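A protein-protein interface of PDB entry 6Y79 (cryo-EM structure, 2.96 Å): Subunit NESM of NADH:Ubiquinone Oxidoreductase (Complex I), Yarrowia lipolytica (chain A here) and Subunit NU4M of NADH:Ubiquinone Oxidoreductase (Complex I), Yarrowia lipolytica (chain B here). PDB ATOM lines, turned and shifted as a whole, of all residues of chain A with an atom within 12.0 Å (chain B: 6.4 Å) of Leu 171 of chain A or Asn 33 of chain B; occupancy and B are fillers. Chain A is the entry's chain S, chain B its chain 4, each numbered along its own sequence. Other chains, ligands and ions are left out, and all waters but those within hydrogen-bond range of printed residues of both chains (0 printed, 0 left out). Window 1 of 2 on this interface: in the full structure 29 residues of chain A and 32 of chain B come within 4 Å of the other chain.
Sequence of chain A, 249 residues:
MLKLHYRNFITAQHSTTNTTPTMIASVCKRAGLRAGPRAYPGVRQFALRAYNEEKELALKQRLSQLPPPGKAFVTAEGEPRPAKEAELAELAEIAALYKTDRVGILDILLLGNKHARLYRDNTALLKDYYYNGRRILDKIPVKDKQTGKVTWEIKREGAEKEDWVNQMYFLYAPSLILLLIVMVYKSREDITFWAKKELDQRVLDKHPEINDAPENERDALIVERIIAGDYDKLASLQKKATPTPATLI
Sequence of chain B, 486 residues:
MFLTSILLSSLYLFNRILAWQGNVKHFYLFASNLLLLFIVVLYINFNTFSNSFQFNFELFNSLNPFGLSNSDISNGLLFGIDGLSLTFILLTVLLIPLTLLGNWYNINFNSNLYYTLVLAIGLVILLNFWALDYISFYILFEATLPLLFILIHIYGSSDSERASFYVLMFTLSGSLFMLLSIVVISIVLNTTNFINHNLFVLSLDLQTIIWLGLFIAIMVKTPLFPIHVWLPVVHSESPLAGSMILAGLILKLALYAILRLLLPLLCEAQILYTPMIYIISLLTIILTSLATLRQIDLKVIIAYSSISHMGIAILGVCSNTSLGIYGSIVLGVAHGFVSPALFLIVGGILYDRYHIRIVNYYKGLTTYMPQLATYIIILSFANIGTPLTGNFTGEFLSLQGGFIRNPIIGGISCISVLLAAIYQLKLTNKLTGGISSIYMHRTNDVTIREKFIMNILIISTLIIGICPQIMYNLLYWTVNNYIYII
Leu 171 of chain A touches just one residue of chain B: Asn 33. Asn 33 of chain B touches just these residues of chain A: Gln 167 (3.1 Å), Met 168 (3.8 Å), Leu 171 (3.7 Å) and Tyr 172 (3.2 Å). Leu 29 of chain B touches just one residue of chain A: Gln 167. Of chain A, only Gln 167 (3.4 Å) comes within 4 Å of Phe 30 of chain B. Ala 31 of chain B touches none of the printed residues of chain A. Ser 32 of chain B touches none of the printed residues of chain A. No residue of chain A comes within 4 Å of Leu 34 of chain B. No residue of chain A comes within 4 Å of Leu 35 of chain B. Of the printed residues of chain A, Leu 36 of chain B touches Tyr 172 and Ser 175. No residue of chain A comes within 4 Å of Leu 37 of chain B. Pro 97 of chain B touches one residue of chain A. Printed residues of chain B within 4 Å of Tyr 172 of chain A: Asn 33 (3.2 Å), Leu 36 (3.4 Å) and Pro 97 (3.7 Å). Of the printed residues of chain B, Ser 175 of chain A touches Leu 36. Of the printed residues of chain B, Gln 167 of chain A touches Leu 29, Phe 30 and Asn 33. Printed residues of chain B within 4 Å of Met 168 of chain A: Asn 33 (3.8 Å). Asn 166 of chain A touches none of the printed residues of chain B. The nearest residue of chain B that does not touch Leu 171 of chain A is Leu 37 of chain B (4.3 Å).
Among the printed residues, pairs that only touch across the chains: Tyr 172 of chain A with Asn 33 of chain B (3.2 Å), Ser 175 of chain A with Leu 36 of chain B (3.3 Å), Gln 167 of chain A with Phe 30 of chain B (3.4 Å), Gln 167 of chain A with Leu 29 of chain B (3.4 Å), Tyr 172 of chain A with Leu 36 of chain B (3.4 Å), Leu 171 of chain A with Asn 33 of chain B (3.7 Å), Tyr 172 of chain A with Pro 97 of chain B (3.7 Å) and Met 168 of chain A with Asn 33 of chain B (3.8 Å).
Of the 20 printed residues of chain A, 5 touch a printed residue of chain B. Hydrophobic or aromatic side chains of chain A within 4 Å of the printed part of chain B: Met 168, Leu 171 and Tyr 172. Hydrophobic or aromatic side chains of chain B within 4 Å of the printed part of chain A: Leu 29, Phe 30, Leu 36 and Pro 97. Among the printed residues, 9 pairs touch across the chains.
O of Leu 171 of chain A is in hydrogen-bond range of OG of Ser 175 of chain A (2.9 Å). O of Leu 29 of chain B lies within hydrogen-bond range of ND2 of Asn 33 of chain B. O of Met 168 of chain A lies within hydrogen-bond range of N of Ala 173 of chain A, at 3.0 Å. O of Gln 167 of chain A is in hydrogen-bond range of N of Tyr 172 of chain A, at 3.5 Å. The backbone carbonyl oxygen (O) of Tyr 172 of chain A is in hydrogen-bond range of the side-chain hydroxyl (OG) of Ser 175 of chain A (2.5 Å).
O of Gln 167 of chain A sits at hydrogen-bond distance from ND2 of Asn 33 of chain B, 3.1 Å away.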
ATOM      1  N   LYS A 161      25.788  34.264  -8.897  1.00  0.00           N
ATOM      2  CA  LYS A 161      25.972  32.861  -9.240  1.00  0.00           C
ATOM      3  C   LYS A 161      26.716  32.781 -10.563  1.00  0.00           C
ATOM      4  O   LYS A 161      26.209  33.246 -11.589  1.00  0.00           O
ATOM      5  CB  LYS A 161      24.635  32.134  -9.349  1.00  0.00           C
ATOM      6  CG  LYS A 161      23.833  32.085  -8.070  1.00  0.00           C
ATOM      7  CD  LYS A 161      22.498  31.414  -8.312  1.00  0.00           C
ATOM      8  CE  LYS A 161      22.686  29.931  -8.521  1.00  0.00           C
ATOM      9  NZ  LYS A 161      23.225  29.267  -7.309  1.00  0.00           N
ATOM     10  N   GLU A 162      27.917  32.211 -10.533  1.00  0.00           N
ATOM     11  CA  GLU A 162      28.629  31.888 -11.758  1.00  0.00           C
ATOM     12  C   GLU A 162      28.068  30.605 -12.372  1.00  0.00           C
ATOM     13  O   GLU A 162      27.309  29.865 -11.745  1.00  0.00           O
ATOM     14  CB  GLU A 162      30.129  31.800 -11.486  1.00  0.00           C
ATOM     15  CG  GLU A 162      30.709  33.169 -11.210  1.00  0.00           C
ATOM     16  CD  GLU A 162      32.205  33.150 -11.074  1.00  0.00           C
ATOM     17  OE1 GLU A 162      32.779  32.048 -11.148  1.00  0.00           O
ATOM     18  OE2 GLU A 162      32.803  34.231 -10.882  1.00  0.00           O
ATOM     19  N   ASP A 163      28.468  30.346 -13.620  1.00  0.00           N
ATOM     20  CA  ASP A 163      27.771  29.405 -14.495  1.00  0.00           C
ATOM     21  C   ASP A 163      27.878  27.957 -14.044  1.00  0.00           C
ATOM     22  O   ASP A 163      27.027  27.141 -14.414  1.00  0.00           O
ATOM     23  CB  ASP A 163      28.323  29.524 -15.911  1.00  0.00           C
ATOM     24  CG  ASP A 163      28.531  30.952 -16.324  1.00  0.00           C
ATOM     25  OD1 ASP A 163      27.631  31.775 -16.057  1.00  0.00           O
ATOM     26  OD2 ASP A 163      29.591  31.258 -16.904  1.00  0.00           O
ATOM     27  N   TRP A 164      28.890  27.619 -13.263  1.00  0.00           N
ATOM     28  CA  TRP A 164      29.109  26.237 -12.885  1.00  0.00           C
ATOM     29  C   TRP A 164      28.419  25.851 -11.586  1.00  0.00           C
ATOM     30  O   TRP A 164      28.261  24.654 -11.326  1.00  0.00           O
ATOM     31  CB  TRP A 164      30.612  25.970 -12.768  1.00  0.00           C
ATOM     32  CG  TRP A 164      31.273  26.811 -11.729  1.00  0.00           C
ATOM     33  CD1 TRP A 164      31.837  28.033 -11.902  1.00  0.00           C
ATOM     34  CD2 TRP A 164      31.424  26.491 -10.343  1.00  0.00           C
ATOM     35  NE1 TRP A 164      32.327  28.497 -10.711  1.00  0.00           N
ATOM     36  CE2 TRP A 164      32.084  27.564  -9.739  1.00  0.00           C
ATOM     37  CE3 TRP A 164      31.057  25.399  -9.555  1.00  0.00           C
ATOM     38  CZ2 TRP A 164      32.376  27.583  -8.391  1.00  0.00           C
ATOM     39  CZ3 TRP A 164      31.355  25.416  -8.228  1.00  0.00           C
ATOM     40  CH2 TRP A 164      32.016  26.495  -7.654  1.00  0.00           C
ATOM     41  N   VAL A 165      28.004  26.818 -10.762  1.00  0.00           N
ATOM     42  CA  VAL A 165      27.540  26.502  -9.412  1.00  0.00           C
ATOM     43  C   VAL A 165      26.163  25.865  -9.385  1.00  0.00           C
ATOM     44  O   VAL A 165      25.743  25.378  -8.333  1.00  0.00           O
ATOM     45  CB  VAL A 165      27.523  27.745  -8.496  1.00  0.00           C
ATOM     46  CG1 VAL A 165      28.811  28.523  -8.616  1.00  0.00           C
ATOM     47  CG2 VAL A 165      26.335  28.627  -8.789  1.00  0.00           C
ATOM     48  N   ASN A 166      25.455  25.847 -10.512  1.00  0.00           N
ATOM     49  CA  ASN A 166      24.130  25.242 -10.547  1.00  0.00           C
ATOM     50  C   ASN A 166      24.216  23.726 -10.486  1.00  0.00           C
ATOM     51  O   ASN A 166      23.435  23.083  -9.782  1.00  0.00           O
ATOM     52  CB  ASN A 166      23.388  25.683 -11.805  1.00  0.00           C
ATOM     53  CG  ASN A 166      22.952  27.129 -11.745  1.00  0.00           C
ATOM     54  OD1 ASN A 166      22.391  27.574 -10.750  1.00  0.00           O
ATOM     55  ND2 ASN A 166      23.213  27.872 -12.814  1.00  0.00           N
ATOM     56  N   GLN A 167      25.156  23.134 -11.220  1.00  0.00           N
ATOM     57  CA  GLN A 167      25.246  21.684 -11.314  1.00  0.00           C
ATOM     58  C   GLN A 167      26.506  21.122 -10.680  1.00  0.00           C
ATOM     59  O   GLN A 167      26.856  19.970 -10.937  1.00  0.00           O
ATOM     60  CB  GLN A 167      25.148  21.232 -12.767  1.00  0.00           C
ATOM     61  CG  GLN A 167      26.200  21.800 -13.679  1.00  0.00           C
ATOM     62  CD  GLN A 167      25.884  21.507 -15.123  1.00  0.00           C
ATOM     63  OE1 GLN A 167      24.994  20.714 -15.420  1.00  0.00           O
ATOM     64  NE2 GLN A 167      26.597  22.155 -16.031  1.00  0.00           N
ATOM     65  N   MET A 168      27.197  21.904  -9.860  1.00  0.00           N
ATOM     66  CA  MET A 168      28.245  21.354  -9.017  1.00  0.00           C
ATOM     67  C   MET A 168      27.864  21.315  -7.552  1.00  0.00           C
ATOM     68  O   MET A 168      28.318  20.426  -6.833  1.00  0.00           O
ATOM     69  CB  MET A 168      29.548  22.143  -9.181  1.00  0.00           C
ATOM     70  CG  MET A 168      30.167  22.035 -10.566  1.00  0.00           C
ATOM     71  SD  MET A 168      30.465  20.354 -11.133  1.00  0.00           S
ATOM     72  CE  MET A 168      31.985  19.968 -10.287  1.00  0.00           C
ATOM     73  N   TYR A 169      27.030  22.246  -7.096  1.00  0.00           N
ATOM     74  CA  TYR A 169      26.544  22.184  -5.726  1.00  0.00           C
ATOM     75  C   TYR A 169      25.278  21.361  -5.612  1.00  0.00           C
ATOM     76  O   TYR A 169      25.007  20.796  -4.549  1.00  0.00           O
ATOM     77  CB  TYR A 169      26.293  23.585  -5.186  1.00  0.00           C
ATOM     78  CG  TYR A 169      27.551  24.364  -4.932  1.00  0.00           C
ATOM     79  CD1 TYR A 169      28.301  24.149  -3.792  1.00  0.00           C
ATOM     80  CD2 TYR A 169      27.985  25.315  -5.832  1.00  0.00           C
ATOM     81  CE1 TYR A 169      29.449  24.864  -3.557  1.00  0.00           C
ATOM     82  CE2 TYR A 169      29.127  26.036  -5.606  1.00  0.00           C
ATOM     83  CZ  TYR A 169      29.857  25.806  -4.467  1.00  0.00           C
ATOM     84  OH  TYR A 169      31.007  26.525  -4.238  1.00  0.00           O
ATOM     85  N   PHE A 170      24.495  21.281  -6.683  1.00  0.00           N
ATOM     86  CA  PHE A 170      23.212  20.604  -6.637  1.00  0.00           C
ATOM     87  C   PHE A 170      23.205  19.270  -7.358  1.00  0.00           C
ATOM     88  O   PHE A 170      22.228  18.528  -7.225  1.00  0.00           O
ATOM     89  CB  PHE A 170      22.116  21.505  -7.218  1.00  0.00           C
ATOM     90  CG  PHE A 170      21.876  22.746  -6.413  1.00  0.00           C
ATOM     91  CD1 PHE A 170      21.156  22.689  -5.236  1.00  0.00           C
ATOM     92  CD2 PHE A 170      22.389  23.963  -6.823  1.00  0.00           C
ATOM     93  CE1 PHE A 170      20.942  23.823  -4.488  1.00  0.00           C
ATOM     94  CE2 PHE A 170      22.180  25.101  -6.080  1.00  0.00           C
ATOM     95  CZ  PHE A 170      21.454  25.031  -4.912  1.00  0.00           C
ATOM     96  N   LEU A 171      24.243  18.947  -8.125  1.00  0.00           N
ATOM     97  CA  LEU A 171      24.360  17.615  -8.705  1.00  0.00           C
ATOM     98  C   LEU A 171      25.652  16.904  -8.332  1.00  0.00           C
ATOM     99  O   LEU A 171      25.605  15.732  -7.955  1.00  0.00           O
ATOM    100  CB  LEU A 171      24.213  17.684 -10.228  1.00  0.00           C
ATOM    101  CG  LEU A 171      24.038  16.331 -10.919  1.00  0.00           C
ATOM    102  CD1 LEU A 171      23.044  15.431 -10.197  1.00  0.00           C
ATOM    103  CD2 LEU A 171      23.601  16.548 -12.349  1.00  0.00           C
ATOM    104  N   TYR A 172      26.807  17.566  -8.444  1.00  0.00           N
ATOM    105  CA  TYR A 172      28.079  16.916  -8.134  1.00  0.00           C
ATOM    106  C   TYR A 172      28.202  16.633  -6.643  1.00  0.00           C
ATOM    107  O   TYR A 172      28.533  15.514  -6.233  1.00  0.00           O
ATOM    108  CB  TYR A 172      29.245  17.788  -8.608  1.00  0.00           C
ATOM    109  CG  TYR A 172      30.615  17.180  -8.401  1.00  0.00           C
ATOM    110  CD1 TYR A 172      31.159  16.346  -9.348  1.00  0.00           C
ATOM    111  CD2 TYR A 172      31.373  17.459  -7.272  1.00  0.00           C
ATOM    112  CE1 TYR A 172      32.394  15.767  -9.175  1.00  0.00           C
ATOM    113  CE2 TYR A 172      32.611  16.888  -7.095  1.00  0.00           C
ATOM    114  CZ  TYR A 172      33.116  16.047  -8.053  1.00  0.00           C
ATOM    115  OH  TYR A 172      34.345  15.471  -7.896  1.00  0.00           O
ATOM    116  N   ALA A 173      27.955  17.647  -5.820  1.00  0.00           N
ATOM    117  CA  ALA A 173      28.139  17.513  -4.377  1.00  0.00           C
ATOM    118  C   ALA A 173      27.158  16.551  -3.701  1.00  0.00           C
ATOM    119  O   ALA A 173      27.608  15.770  -2.842  1.00  0.00           O
ATOM    120  CB  ALA A 173      28.117  18.908  -3.743  1.00  0.00           C
ATOM    121  N   PRO A 174      25.846  16.526  -4.011  1.00  0.00           N
ATOM    122  CA  PRO A 174      25.025  15.463  -3.418  1.00  0.00           C
ATOM    123  C   PRO A 174      25.318  14.080  -3.963  1.00  0.00           C
ATOM    124  O   PRO A 174      25.134  13.109  -3.228  1.00  0.00           O
ATOM    125  CB  PRO A 174      23.592  15.904  -3.737  1.00  0.00           C
ATOM    126  CG  PRO A 174      23.725  16.717  -4.903  1.00  0.00           C
ATOM    127  CD  PRO A 174      24.955  17.499  -4.673  1.00  0.00           C
ATOM    128  N   SER A 175      25.780  13.954  -5.209  1.00  0.00           N
ATOM    129  CA  SER A 175      26.209  12.646  -5.692  1.00  0.00           C
ATOM    130  C   SER A 175      27.455  12.168  -4.964  1.00  0.00           C
ATOM    131  O   SER A 175      27.598  10.972  -4.698  1.00  0.00           O
ATOM    132  CB  SER A 175      26.472  12.696  -7.186  1.00  0.00           C
ATOM    133  OG  SER A 175      27.540  13.578  -7.444  1.00  0.00           O
ATOM    134  N   LEU A 176      28.344  13.088  -4.598  1.00  0.00           N
ATOM    135  CA  LEU A 176      29.547  12.714  -3.865  1.00  0.00           C
ATOM    136  C   LEU A 176      29.229  12.345  -2.418  1.00  0.00           C
ATOM    137  O   LEU A 176      29.800  11.392  -1.872  1.00  0.00           O
ATOM    138  CB  LEU A 176      30.546  13.862  -3.941  1.00  0.00           C
ATOM    139  CG  LEU A 176      32.022  13.515  -3.887  1.00  0.00           C
ATOM    140  CD1 LEU A 176      32.362  12.383  -4.828  1.00  0.00           C
ATOM    141  CD2 LEU A 176      32.831  14.743  -4.220  1.00  0.00           C
ATOM    142  N   ILE A 177      28.307  13.078  -1.787  1.00  0.00           N
ATOM    143  CA  ILE A 177      27.847  12.709  -0.448  1.00  0.00           C
ATOM    144  C   ILE A 177      27.078  11.392  -0.491  1.00  0.00           C
ATOM    145  O   ILE A 177      27.180  10.572   0.433  1.00  0.00           O
ATOM    146  CB  ILE A 177      27.012  13.863   0.142  1.00  0.00           C
ATOM    147  CG1 ILE A 177      27.895  15.072   0.392  1.00  0.00           C
ATOM    148  CG2 ILE A 177      26.328  13.482   1.445  1.00  0.00           C
ATOM    149  CD1 ILE A 177      27.126  16.340   0.573  1.00  0.00           C
ATOM    150  N   LEU A 178      26.341  11.147  -1.576  1.00  0.00           N
ATOM    151  CA  LEU A 178      25.695   9.860  -1.785  1.00  0.00           C
ATOM    152  C   LEU A 178      26.728   8.746  -1.860  1.00  0.00           C
ATOM    153  O   LEU A 178      26.557   7.728  -1.200  1.00  0.00           O
ATOM    154  CB  LEU A 178      24.840   9.909  -3.064  1.00  0.00           C
ATOM    155  CG  LEU A 178      23.639   8.955  -3.250  1.00  0.00           C
ATOM    156  CD1 LEU A 178      22.590   9.605  -4.130  1.00  0.00           C
ATOM    157  CD2 LEU A 178      24.023   7.596  -3.860  1.00  0.00           C
ATOM    158  N   LEU A 179      27.817   8.956  -2.606  1.00  0.00           N
ATOM    159  CA  LEU A 179      28.918   7.997  -2.700  1.00  0.00           C
ATOM    160  C   LEU A 179      29.515   7.692  -1.335  1.00  0.00           C
ATOM    161  O   LEU A 179      29.796   6.529  -1.032  1.00  0.00           O
ATOM    162  CB  LEU A 179      29.997   8.540  -3.641  1.00  0.00           C
ATOM    163  CG  LEU A 179      31.153   7.664  -4.157  1.00  0.00           C
ATOM    164  CD1 LEU A 179      31.468   8.029  -5.574  1.00  0.00           C
ATOM    165  CD2 LEU A 179      32.385   7.879  -3.345  1.00  0.00           C
ATOM    166  N   LEU A 180      29.690   8.726  -0.502  1.00  0.00           N
ATOM    167  CA  LEU A 180      30.159   8.535   0.874  1.00  0.00           C
ATOM    168  C   LEU A 180      29.215   7.650   1.676  1.00  0.00           C
ATOM    169  O   LEU A 180      29.655   6.728   2.370  1.00  0.00           O
ATOM    170  CB  LEU A 180      30.307   9.889   1.569  1.00  0.00           C
ATOM    171  CG  LEU A 180      30.916  10.000   2.976  1.00  0.00           C
ATOM    172  CD1 LEU A 180      31.594  11.311   3.061  1.00  0.00           C
ATOM    173  CD2 LEU A 180      29.915   9.933   4.128  1.00  0.00           C
ATOM    174  N   TYR B  28      28.848  19.238 -21.091  1.00  0.00           N
ATOM    175  CA  TYR B  28      29.890  18.285 -20.734  1.00  0.00           C
ATOM    176  C   TYR B  28      29.950  18.093 -19.227  1.00  0.00           C
ATOM    177  O   TYR B  28      30.113  16.965 -18.747  1.00  0.00           O
ATOM    178  CB  TYR B  28      31.242  18.742 -21.265  1.00  0.00           C
ATOM    179  CG  TYR B  28      31.439  18.518 -22.733  1.00  0.00           C
ATOM    180  CD1 TYR B  28      30.547  17.741 -23.478  1.00  0.00           C
ATOM    181  CD2 TYR B  28      32.552  19.002 -23.359  1.00  0.00           C
ATOM    182  CE1 TYR B  28      30.750  17.532 -24.825  1.00  0.00           C
ATOM    183  CE2 TYR B  28      32.743  18.814 -24.686  1.00  0.00           C
ATOM    184  CZ  TYR B  28      31.887  18.069 -25.410  1.00  0.00           C
ATOM    185  OH  TYR B  28      32.137  17.866 -26.744  1.00  0.00           O
ATOM    186  N   LEU B  29      29.792  19.183 -18.466  1.00  0.00           N
ATOM    187  CA  LEU B  29      29.654  19.077 -17.016  1.00  0.00           C
ATOM    188  C   LEU B  29      28.427  18.267 -16.632  1.00  0.00           C
ATOM    189  O   LEU B  29      28.474  17.455 -15.698  1.00  0.00           O
ATOM    190  CB  LEU B  29      29.551  20.461 -16.385  1.00  0.00           C
ATOM    191  CG  LEU B  29      30.748  21.305 -15.977  1.00  0.00           C
ATOM    192  CD1 LEU B  29      30.233  22.328 -14.995  1.00  0.00           C
ATOM    193  CD2 LEU B  29      31.831  20.477 -15.352  1.00  0.00           C
ATOM    194  N   PHE B  30      27.319  18.487 -17.338  1.00  0.00           N
ATOM    195  CA  PHE B  30      26.077  17.790 -17.033  1.00  0.00           C
ATOM    196  C   PHE B  30      26.198  16.296 -17.300  1.00  0.00           C
ATOM    197  O   PHE B  30      25.787  15.475 -16.471  1.00  0.00           O
ATOM    198  CB  PHE B  30      24.951  18.409 -17.854  1.00  0.00           C
ATOM    199  CG  PHE B  30      23.617  17.821 -17.583  1.00  0.00           C
ATOM    200  CD1 PHE B  30      22.991  18.030 -16.369  1.00  0.00           C
ATOM    201  CD2 PHE B  30      22.979  17.060 -18.543  1.00  0.00           C
ATOM    202  CE1 PHE B  30      21.755  17.484 -16.113  1.00  0.00           C
ATOM    203  CE2 PHE B  30      21.740  16.514 -18.294  1.00  0.00           C
ATOM    204  CZ  PHE B  30      21.129  16.724 -17.078  1.00  0.00           C
ATOM    205  N   ALA B  31      26.806  15.928 -18.431  1.00  0.00           N
ATOM    206  CA  ALA B  31      27.029  14.526 -18.757  1.00  0.00           C
ATOM    207  C   ALA B  31      28.027  13.881 -17.806  1.00  0.00           C
ATOM    208  O   ALA B  31      27.883  12.701 -17.465  1.00  0.00           O
ATOM    209  CB  ALA B  31      27.501  14.399 -20.201  1.00  0.00           C
ATOM    210  N   SER B  32      29.014  14.649 -17.334  1.00  0.00           N
ATOM    211  CA  SER B  32      29.966  14.116 -16.370  1.00  0.00           C
ATOM    212  C   SER B  32      29.300  13.812 -15.038  1.00  0.00           C
ATOM    213  O   SER B  32      29.548  12.760 -14.442  1.00  0.00           O
ATOM    214  CB  SER B  32      31.093  15.109 -16.174  1.00  0.00           C
ATOM    215  OG  SER B  32      31.661  15.432 -17.421  1.00  0.00           O
ATOM    216  N   ASN B  33      28.437  14.703 -14.560  1.00  0.00           N
ATOM    217  CA  ASN B  33      27.779  14.457 -13.280  1.00  0.00           C
ATOM    218  C   ASN B  33      26.699  13.386 -13.393  1.00  0.00           C
ATOM    219  O   ASN B  33      26.453  12.651 -12.426  1.00  0.00           O
ATOM    220  CB  ASN B  33      27.229  15.769 -12.745  1.00  0.00           C
ATOM    221  CG  ASN B  33      28.310  16.795 -12.562  1.00  0.00           C
ATOM    222  OD1 ASN B  33      29.388  16.487 -12.060  1.00  0.00           O
ATOM    223  ND2 ASN B  33      28.046  18.014 -12.991  1.00  0.00           N
ATOM    224  N   LEU B  34      26.065  13.260 -14.565  1.00  0.00           N
ATOM    225  CA  LEU B  34      25.188  12.119 -14.812  1.00  0.00           C
ATOM    226  C   LEU B  34      25.955  10.809 -14.797  1.00  0.00           C
ATOM    227  O   LEU B  34      25.448   9.800 -14.293  1.00  0.00           O
ATOM    228  CB  LEU B  34      24.487  12.264 -16.152  1.00  0.00           C
ATOM    229  CG  LEU B  34      23.356  13.265 -16.320  1.00  0.00           C
ATOM    230  CD1 LEU B  34      22.799  13.105 -17.715  1.00  0.00           C
ATOM    231  CD2 LEU B  34      22.286  13.056 -15.274  1.00  0.00           C
ATOM    232  N   LEU B  35      27.169  10.810 -15.349  1.00  0.00           N
ATOM    233  CA  LEU B  35      28.007   9.619 -15.327  1.00  0.00           C
ATOM    234  C   LEU B  35      28.416   9.259 -13.905  1.00  0.00           C
ATOM    235  O   LEU B  35      28.467   8.073 -13.550  1.00  0.00           O
ATOM    236  CB  LEU B  35      29.227   9.860 -16.207  1.00  0.00           C
ATOM    237  CG  LEU B  35      30.263   8.761 -16.292  1.00  0.00           C
ATOM    238  CD1 LEU B  35      29.713   7.592 -17.058  1.00  0.00           C
ATOM    239  CD2 LEU B  35      31.481   9.335 -16.950  1.00  0.00           C
ATOM    240  N   LEU B  36      28.706  10.277 -13.087  1.00  0.00           N
ATOM    241  CA  LEU B  36      28.906  10.086 -11.652  1.00  0.00           C
ATOM    242  C   LEU B  36      27.735   9.379 -11.003  1.00  0.00           C
ATOM    243  O   LEU B  36      27.923   8.347 -10.354  1.00  0.00           O
ATOM    244  CB  LEU B  36      29.090  11.408 -10.945  1.00  0.00           C
ATOM    245  CG  LEU B  36      30.355  12.115 -10.582  1.00  0.00           C
ATOM    246  CD1 LEU B  36      29.758  13.249  -9.889  1.00  0.00           C
ATOM    247  CD2 LEU B  36      31.165  11.312  -9.608  1.00  0.00           C
ATOM    248  N   LEU B  37      26.523   9.931 -11.160  1.00  0.00           N
ATOM    249  CA  LEU B  37      25.346   9.356 -10.512  1.00  0.00           C
ATOM    250  C   LEU B  37      25.089   7.939 -10.998  1.00  0.00           C
ATOM    251  O   LEU B  37      24.697   7.074 -10.211  1.00  0.00           O
ATOM    252  CB  LEU B  37      24.113  10.241 -10.749  1.00  0.00           C
ATOM    253  CG  LEU B  37      22.830   9.996  -9.916  1.00  0.00           C
ATOM    254  CD1 LEU B  37      22.130  11.313  -9.655  1.00  0.00           C
ATOM    255  CD2 LEU B  37      21.826   9.032 -10.554  1.00  0.00           C
ATOM    256  N   PHE B  38      25.357   7.675 -12.278  1.00  0.00           N
ATOM    257  CA  PHE B  38      25.175   6.335 -12.827  1.00  0.00           C
ATOM    258  C   PHE B  38      26.144   5.336 -12.214  1.00  0.00           C
ATOM    259  O   PHE B  38      25.746   4.221 -11.863  1.00  0.00           O
ATOM    260  CB  PHE B  38      25.346   6.359 -14.343  1.00  0.00           C
ATOM    261  CG  PHE B  38      25.156   5.023 -14.990  1.00  0.00           C
ATOM    262  CD1 PHE B  38      23.885   4.483 -15.115  1.00  0.00           C
ATOM    263  CD2 PHE B  38      26.240   4.288 -15.432  1.00  0.00           C
ATOM    264  CE1 PHE B  38      23.702   3.242 -15.682  1.00  0.00           C
ATOM    265  CE2 PHE B  38      26.060   3.045 -15.997  1.00  0.00           C
ATOM    266  CZ  PHE B  38      24.787   2.523 -16.123  1.00  0.00           C
ATOM    267  N   PRO B  97      34.629  15.501 -13.920  1.00  0.00           N
ATOM    268  CA  PRO B  97      34.060  16.856 -13.811  1.00  0.00           C
ATOM    269  C   PRO B  97      35.021  17.887 -13.273  1.00  0.00           C
ATOM    270  O   PRO B  97      34.911  19.056 -13.646  1.00  0.00           O
ATOM    271  CB  PRO B  97      32.887  16.674 -12.843  1.00  0.00           C
ATOM    272  CG  PRO B  97      32.587  15.285 -12.862  1.00  0.00           C
ATOM    273  CD  PRO B  97      33.862  14.593 -13.044  1.00  0.00           C
